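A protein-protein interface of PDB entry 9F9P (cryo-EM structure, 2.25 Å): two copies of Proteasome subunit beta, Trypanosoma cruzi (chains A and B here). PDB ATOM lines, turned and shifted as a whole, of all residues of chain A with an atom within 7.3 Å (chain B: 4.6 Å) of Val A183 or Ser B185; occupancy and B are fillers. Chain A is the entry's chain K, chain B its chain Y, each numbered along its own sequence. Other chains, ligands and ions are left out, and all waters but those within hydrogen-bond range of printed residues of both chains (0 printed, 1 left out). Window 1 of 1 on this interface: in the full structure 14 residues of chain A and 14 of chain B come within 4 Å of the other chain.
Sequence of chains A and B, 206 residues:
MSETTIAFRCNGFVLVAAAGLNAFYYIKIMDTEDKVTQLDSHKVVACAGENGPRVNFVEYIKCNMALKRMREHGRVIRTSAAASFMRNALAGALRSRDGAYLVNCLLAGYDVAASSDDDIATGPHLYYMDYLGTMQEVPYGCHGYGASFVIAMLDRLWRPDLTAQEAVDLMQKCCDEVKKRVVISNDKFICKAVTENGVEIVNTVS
Val A183 touches Ile B184, and with the chains exchanged Ile A184 touches Val B183. Val A183 touches Ser B185, and with the chains exchanged Ser A185 touches Val B183. Ile B184 touches its own counterpart, Ile A184. 4 positions are printed for both chains.
Of the 10 printed residues of chain A, 8 touch a printed residue of chain B. Among the printed residues, 18 pairs touch across the chains.
Among the printed residues, pairs that only touch across the chains: Tyr A145 with Tyr B26, Lys A179 with Lys B28, Lys A180 with Lys B28, Arg A181 with Tyr B26, Arg A181 with Ile B27, Val A182 with Tyr B26, Val A182 with Lys B28, Val A183 with Ala B23, Val A183 with Tyr B25, Val A183 with Ile B27, Val A183 with Lys B28, Val A183 with Ile B184, Ile A184 with Val B183 and Ile A184 with Ile B184.
The guanidinium group of Arg A181 sits at hydrogen-bond distance from the backbone carbonyl oxygen of Lys B28 (2.7 Å). The backbone NH (N) of Val A183 lies within hydrogen-bond range of the backbone carbonyl oxygen (O) of Tyr B26, at 2.8 Å. The backbone NH of Ser B185 is in hydrogen-bond range of the backbone carbonyl oxygen of Val A183 (3.1 Å). The backbone carbonyl oxygen (O) of Val B183 is in hydrogen-bond range of the backbone NH (N) of Ser A185 (3.1 Å).
The side-chain hydroxyl of Ser B185 lies within hydrogen-bond range of the side-chain amino group of Lys B28 (3.3 Å).
Val A183 touches seven residues of chain B. Of chain A, only Val A183 (3.1 Å) comes within 4 Å of Ser B185. Of the printed residues of chain A, Tyr B26 touches Tyr A145 (3.8 Å), Arg A181 (3.9 Å), Val A182 (3.7 Å) and Val A183 (2.8 Å). Of the printed residues of chain A, Ile B184 touches Val A183 and Ile A184. Of the printed residues of chain B, Tyr A145 touches Tyr B26 (3.8 Å). Printed residues of chain B within 4 Å of Arg A181: Tyr B26 (3.9 Å), Ile B27 (3.6 Å) and Lys B28 (2.7 Å). Asp B187 touches none of the printed residues of chain A. Leu B21 touches none of the printed residues of chain A. The nearest residue of chain B that does not touch Val A183 is Val B183 (4.1 Å). The nearest residue of chain A that does not touch Ser B185 is Ser A185 (4.5 Å). The nearest printed residue of chain B that does not touch Ser A185 is Ser B185 (4.5 Å).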
ATOM      1  N   TYR A 145     -17.624  33.027  18.715  1.00  0.00           N
ATOM      2  CA  TYR A 145     -17.918  31.709  18.129  1.00  0.00           C
ATOM      3  C   TYR A 145     -17.905  30.611  19.204  1.00  0.00           C
ATOM      4  O   TYR A 145     -18.678  29.689  19.137  1.00  0.00           O
ATOM      5  CB  TYR A 145     -16.935  31.370  16.999  1.00  0.00           C
ATOM      6  CG  TYR A 145     -17.047  32.158  15.718  1.00  0.00           C
ATOM      7  CD1 TYR A 145     -18.248  32.359  15.075  1.00  0.00           C
ATOM      8  CD2 TYR A 145     -15.909  32.657  15.101  1.00  0.00           C
ATOM      9  CE1 TYR A 145     -18.322  33.068  13.878  1.00  0.00           C
ATOM     10  CE2 TYR A 145     -15.953  33.388  13.923  1.00  0.00           C
ATOM     11  CZ  TYR A 145     -17.170  33.584  13.297  1.00  0.00           C
ATOM     12  OH  TYR A 145     -17.192  34.290  12.113  1.00  0.00           O
ATOM     13  N   VAL A 178     -12.900  25.852  24.049  1.00  0.00           N
ATOM     14  CA  VAL A 178     -12.816  26.791  22.936  1.00  0.00           C
ATOM     15  C   VAL A 178     -11.636  26.471  22.025  1.00  0.00           C
ATOM     16  O   VAL A 178     -11.808  26.496  20.813  1.00  0.00           O
ATOM     17  CB  VAL A 178     -12.765  28.245  23.430  1.00  0.00           C
ATOM     18  CG1 VAL A 178     -12.643  29.251  22.282  1.00  0.00           C
ATOM     19  CG2 VAL A 178     -13.979  28.552  24.288  1.00  0.00           C
ATOM     20  N   LYS A 179     -10.473  26.141  22.584  1.00  0.00           N
ATOM     21  CA  LYS A 179      -9.307  25.791  21.777  1.00  0.00           C
ATOM     22  C   LYS A 179      -9.496  24.496  20.996  1.00  0.00           C
ATOM     23  O   LYS A 179      -9.047  24.373  19.867  1.00  0.00           O
ATOM     24  CB  LYS A 179      -8.077  25.556  22.658  1.00  0.00           C
ATOM     25  CG  LYS A 179      -7.581  26.822  23.336  1.00  0.00           C
ATOM     26  CD  LYS A 179      -6.576  26.572  24.450  1.00  0.00           C
ATOM     27  CE  LYS A 179      -6.359  27.818  25.286  1.00  0.00           C
ATOM     28  NZ  LYS A 179      -5.190  27.671  26.181  1.00  0.00           N
ATOM     29  N   LYS A 180     -10.175  23.535  21.625  1.00  0.00           N
ATOM     30  CA  LYS A 180     -10.441  22.251  21.003  1.00  0.00           C
ATOM     31  C   LYS A 180     -11.352  22.395  19.796  1.00  0.00           C
ATOM     32  O   LYS A 180     -11.068  21.769  18.791  1.00  0.00           O
ATOM     33  CB  LYS A 180     -11.066  21.274  21.996  1.00  0.00           C
ATOM     34  CG  LYS A 180     -11.245  19.868  21.440  1.00  0.00           C
ATOM     35  CD  LYS A 180     -11.669  18.860  22.500  1.00  0.00           C
ATOM     36  CE  LYS A 180     -11.213  17.444  22.180  1.00  0.00           C
ATOM     37  NZ  LYS A 180     -12.016  16.857  21.086  1.00  0.00           N
ATOM     38  N   ARG A 181     -12.436  23.188  19.879  1.00  0.00           N
ATOM     39  CA  ARG A 181     -13.502  23.079  18.883  1.00  0.00           C
ATOM     40  C   ARG A 181     -13.636  24.258  17.949  1.00  0.00           C
ATOM     41  O   ARG A 181     -14.406  24.129  17.021  1.00  0.00           O
ATOM     42  CB  ARG A 181     -14.888  22.884  19.518  1.00  0.00           C
ATOM     43  CG  ARG A 181     -15.105  21.502  20.122  1.00  0.00           C
ATOM     44  CD  ARG A 181     -15.449  20.483  19.041  1.00  0.00           C
ATOM     45  NE  ARG A 181     -15.312  19.125  19.519  1.00  0.00           N
ATOM     46  CZ  ARG A 181     -15.123  18.083  18.727  1.00  0.00           C
ATOM     47  NH1 ARG A 181     -14.912  18.272  17.441  1.00  0.00           N
ATOM     48  NH2 ARG A 181     -15.095  16.869  19.224  1.00  0.00           N
ATOM     49  N   VAL A 182     -12.980  25.402  18.158  1.00  0.00           N
ATOM     50  CA  VAL A 182     -13.198  26.542  17.259  1.00  0.00           C
ATOM     51  C   VAL A 182     -12.052  26.680  16.261  1.00  0.00           C
ATOM     52  O   VAL A 182     -10.905  26.666  16.640  1.00  0.00           O
ATOM     53  CB  VAL A 182     -13.417  27.851  18.047  1.00  0.00           C
ATOM     54  CG1 VAL A 182     -13.534  29.070  17.144  1.00  0.00           C
ATOM     55  CG2 VAL A 182     -14.662  27.754  18.904  1.00  0.00           C
ATOM     56  N   VAL A 183     -12.363  26.784  14.983  1.00  0.00           N
ATOM     57  CA  VAL A 183     -11.348  26.819  13.937  1.00  0.00           C
ATOM     58  C   VAL A 183     -10.437  28.028  14.127  1.00  0.00           C
ATOM     59  O   VAL A 183      -9.224  27.866  14.147  1.00  0.00           O
ATOM     60  CB  VAL A 183     -11.988  26.875  12.532  1.00  0.00           C
ATOM     61  CG1 VAL A 183     -11.005  27.323  11.480  1.00  0.00           C
ATOM     62  CG2 VAL A 183     -12.588  25.555  12.127  1.00  0.00           C
ATOM     63  N   ILE A 184     -11.017  29.232  14.248  1.00  0.00           N
ATOM     64  CA  ILE A 184     -10.251  30.430  14.578  1.00  0.00           C
ATOM     65  C   ILE A 184      -9.464  30.225  15.872  1.00  0.00           C
ATOM     66  O   ILE A 184     -10.049  30.009  16.919  1.00  0.00           O
ATOM     67  CB  ILE A 184     -11.155  31.661  14.718  1.00  0.00           C
ATOM     68  CG1 ILE A 184     -12.003  31.944  13.472  1.00  0.00           C
ATOM     69  CG2 ILE A 184     -10.315  32.859  15.111  1.00  0.00           C
ATOM     70  CD1 ILE A 184     -11.218  32.143  12.193  1.00  0.00           C
ATOM     71  N   SER A 185      -8.146  30.365  15.798  1.00  0.00           N
ATOM     72  CA  SER A 185      -7.249  30.119  16.918  1.00  0.00           C
ATOM     73  C   SER A 185      -7.399  31.165  18.034  1.00  0.00           C
ATOM     74  O   SER A 185      -7.111  32.343  17.815  1.00  0.00           O
ATOM     75  CB  SER A 185      -5.804  30.082  16.451  1.00  0.00           C
ATOM     76  OG  SER A 185      -4.929  30.065  17.578  1.00  0.00           O
ATOM     77  N   ASN A 186      -7.800  30.709  19.235  1.00  0.00           N
ATOM     78  CA  ASN A 186      -7.817  31.509  20.452  1.00  0.00           C
ATOM     79  C   ASN A 186      -6.920  30.834  21.477  1.00  0.00           C
ATOM     80  O   ASN A 186      -7.414  30.077  22.298  1.00  0.00           O
ATOM     81  CB  ASN A 186      -9.216  31.616  21.056  1.00  0.00           C
ATOM     82  CG  ASN A 186     -10.139  32.610  20.384  1.00  0.00           C
ATOM     83  OD1 ASN A 186     -11.289  32.760  20.775  1.00  0.00           O
ATOM     84  ND2 ASN A 186      -9.640  33.328  19.393  1.00  0.00           N
ATOM     85  N   LEU B  21      -6.717  19.010   9.442  1.00  0.00           N
ATOM     86  CA  LEU B  21      -7.980  19.598   9.853  1.00  0.00           C
ATOM     87  C   LEU B  21      -9.146  19.281   8.925  1.00  0.00           C
ATOM     88  O   LEU B  21      -9.090  19.599   7.750  1.00  0.00           O
ATOM     89  CB  LEU B  21      -7.788  21.117   9.872  1.00  0.00           C
ATOM     90  CG  LEU B  21      -9.050  21.953  10.108  1.00  0.00           C
ATOM     91  CD1 LEU B  21      -9.417  21.926  11.581  1.00  0.00           C
ATOM     92  CD2 LEU B  21      -8.864  23.392   9.646  1.00  0.00           C
ATOM     93  N   ALA B  23     -13.211  20.696   8.820  1.00  0.00           N
ATOM     94  CA  ALA B  23     -14.042  21.726   9.445  1.00  0.00           C
ATOM     95  C   ALA B  23     -15.415  21.827   8.793  1.00  0.00           C
ATOM     96  O   ALA B  23     -15.569  21.533   7.610  1.00  0.00           O
ATOM     97  CB  ALA B  23     -13.361  23.061   9.318  1.00  0.00           C
ATOM     98  N   TYR B  25     -17.722  25.062   8.593  1.00  0.00           N
ATOM     99  CA  TYR B  25     -17.726  26.483   8.914  1.00  0.00           C
ATOM    100  C   TYR B  25     -16.668  26.722   9.982  1.00  0.00           C
ATOM    101  O   TYR B  25     -15.505  26.418   9.731  1.00  0.00           O
ATOM    102  CB  TYR B  25     -19.141  26.961   9.252  1.00  0.00           C
ATOM    103  CG  TYR B  25     -20.094  26.849   8.090  1.00  0.00           C
ATOM    104  CD1 TYR B  25     -19.918  27.621   6.951  1.00  0.00           C
ATOM    105  CD2 TYR B  25     -21.137  25.933   8.107  1.00  0.00           C
ATOM    106  CE1 TYR B  25     -20.768  27.500   5.864  1.00  0.00           C
ATOM    107  CE2 TYR B  25     -21.998  25.801   7.031  1.00  0.00           C
ATOM    108  CZ  TYR B  25     -21.814  26.588   5.906  1.00  0.00           C
ATOM    109  OH  TYR B  25     -22.670  26.466   4.835  1.00  0.00           O
ATOM    110  N   TYR B  26     -17.083  27.139  11.182  1.00  0.00           N
ATOM    111  CA  TYR B  26     -16.140  27.556  12.201  1.00  0.00           C
ATOM    112  C   TYR B  26     -15.877  26.438  13.204  1.00  0.00           C
ATOM    113  O   TYR B  26     -15.061  26.671  14.072  1.00  0.00           O
ATOM    114  CB  TYR B  26     -16.589  28.882  12.838  1.00  0.00           C
ATOM    115  CG  TYR B  26     -17.913  28.849  13.577  1.00  0.00           C
ATOM    116  CD1 TYR B  26     -18.023  28.298  14.851  1.00  0.00           C
ATOM    117  CD2 TYR B  26     -19.064  29.342  12.981  1.00  0.00           C
ATOM    118  CE1 TYR B  26     -19.240  28.234  15.507  1.00  0.00           C
ATOM    119  CE2 TYR B  26     -20.294  29.290  13.624  1.00  0.00           C
ATOM    120  CZ  TYR B  26     -20.381  28.745  14.897  1.00  0.00           C
ATOM    121  OH  TYR B  26     -21.609  28.703  15.516  1.00  0.00           O
ATOM    122  N   ILE B  27     -16.482  25.240  13.060  1.00  0.00           N
ATOM    123  CA  ILE B  27     -16.313  24.139  14.016  1.00  0.00           C
ATOM    124  C   ILE B  27     -15.262  23.128  13.538  1.00  0.00           C
ATOM    125  O   ILE B  27     -15.392  22.582  12.461  1.00  0.00           O
ATOM    126  CB  ILE B  27     -17.668  23.423  14.279  1.00  0.00           C
ATOM    127  CG1 ILE B  27     -18.746  24.378  14.789  1.00  0.00           C
ATOM    128  CG2 ILE B  27     -17.532  22.266  15.249  1.00  0.00           C
ATOM    129  CD1 ILE B  27     -19.841  24.690  13.787  1.00  0.00           C
ATOM    130  N   LYS B  28     -14.251  22.807  14.346  1.00  0.00           N
ATOM    131  CA  LYS B  28     -13.387  21.669  14.054  1.00  0.00           C
ATOM    132  C   LYS B  28     -14.085  20.335  14.338  1.00  0.00           C
ATOM    133  O   LYS B  28     -14.369  20.033  15.495  1.00  0.00           O
ATOM    134  CB  LYS B  28     -12.097  21.649  14.883  1.00  0.00           C
ATOM    135  CG  LYS B  28     -11.207  22.837  14.625  1.00  0.00           C
ATOM    136  CD  LYS B  28     -10.168  23.154  15.709  1.00  0.00           C
ATOM    137  CE  LYS B  28      -8.919  22.318  15.621  1.00  0.00           C
ATOM    138  NZ  LYS B  28      -7.913  22.817  16.588  1.00  0.00           N
ATOM    139  N   VAL B 183      -4.168  32.420  11.383  1.00  0.00           N
ATOM    140  CA  VAL B 183      -5.320  32.485  12.275  1.00  0.00           C
ATOM    141  C   VAL B 183      -6.060  31.151  12.279  1.00  0.00           C
ATOM    142  O   VAL B 183      -6.308  30.608  13.347  1.00  0.00           O
ATOM    143  CB  VAL B 183      -6.293  33.610  11.855  1.00  0.00           C
ATOM    144  CG1 VAL B 183      -7.656  33.439  12.477  1.00  0.00           C
ATOM    145  CG2 VAL B 183      -5.758  34.977  12.187  1.00  0.00           C
ATOM    146  N   ILE B 184      -6.422  30.636  11.094  1.00  0.00           N
ATOM    147  CA  ILE B 184      -7.001  29.302  10.974  1.00  0.00           C
ATOM    148  C   ILE B 184      -6.083  28.257  11.609  1.00  0.00           C
ATOM    149  O   ILE B 184      -4.958  28.079  11.171  1.00  0.00           O
ATOM    150  CB  ILE B 184      -7.267  28.926   9.511  1.00  0.00           C
ATOM    151  CG1 ILE B 184      -8.171  29.925   8.777  1.00  0.00           C
ATOM    152  CG2 ILE B 184      -7.817  27.518   9.444  1.00  0.00           C
ATOM    153  CD1 ILE B 184      -9.529  30.144   9.405  1.00  0.00           C
ATOM    154  N   SER B 185      -6.597  27.529  12.592  1.00  0.00           N
ATOM    155  CA  SER B 185      -5.829  26.556  13.357  1.00  0.00           C
ATOM    156  C   SER B 185      -5.432  25.329  12.519  1.00  0.00           C
ATOM    157  O   SER B 185      -6.304  24.579  12.078  1.00  0.00           O
ATOM    158  CB  SER B 185      -6.603  26.103  14.582  1.00  0.00           C
ATOM    159  OG  SER B 185      -5.941  24.997  15.195  1.00  0.00           O
ATOM    160  N   ASN B 186      -4.113  25.114  12.355  1.00  0.00           N
ATOM    161  CA  ASN B 186      -3.546  23.913  11.760  1.00  0.00           C
ATOM    162  C   ASN B 186      -2.632  23.261  12.786  1.00  0.00           C
ATOM    163  O   ASN B 186      -1.436  23.501  12.759  1.00  0.00           O
ATOM    164  CB  ASN B 186      -2.711  24.217  10.519  1.00  0.00           C
ATOM    165  CG  ASN B 186      -3.502  24.476   9.253  1.00  0.00           C
ATOM    166  OD1 ASN B 186      -2.932  24.752   8.206  1.00  0.00           O
ATOM    167  ND2 ASN B 186      -4.816  24.356   9.322  1.00  0.00           N
ATOM    168  N   ASP B 187      -3.191  22.466  13.699  1.00  0.00           N
ATOM    169  CA  ASP B 187      -2.495  22.106  14.925  1.00  0.00           C
ATOM    170  C   ASP B 187      -1.692  20.809  14.760  1.00  0.00           C
ATOM    171  O   ASP B 187      -0.640  20.677  15.392  1.00  0.00           O
ATOM    172  CB  ASP B 187      -3.477  22.057  16.103  1.00  0.00           C
ATOM    173  CG  ASP B 187      -2.831  21.938  17.482  1.00  0.00           C
ATOM    174  OD1 ASP B 187      -2.170  22.913  17.921  1.00  0.00           O
ATOM    175  OD2 ASP B 187      -2.992  20.865  18.118  1.00  0.00           O
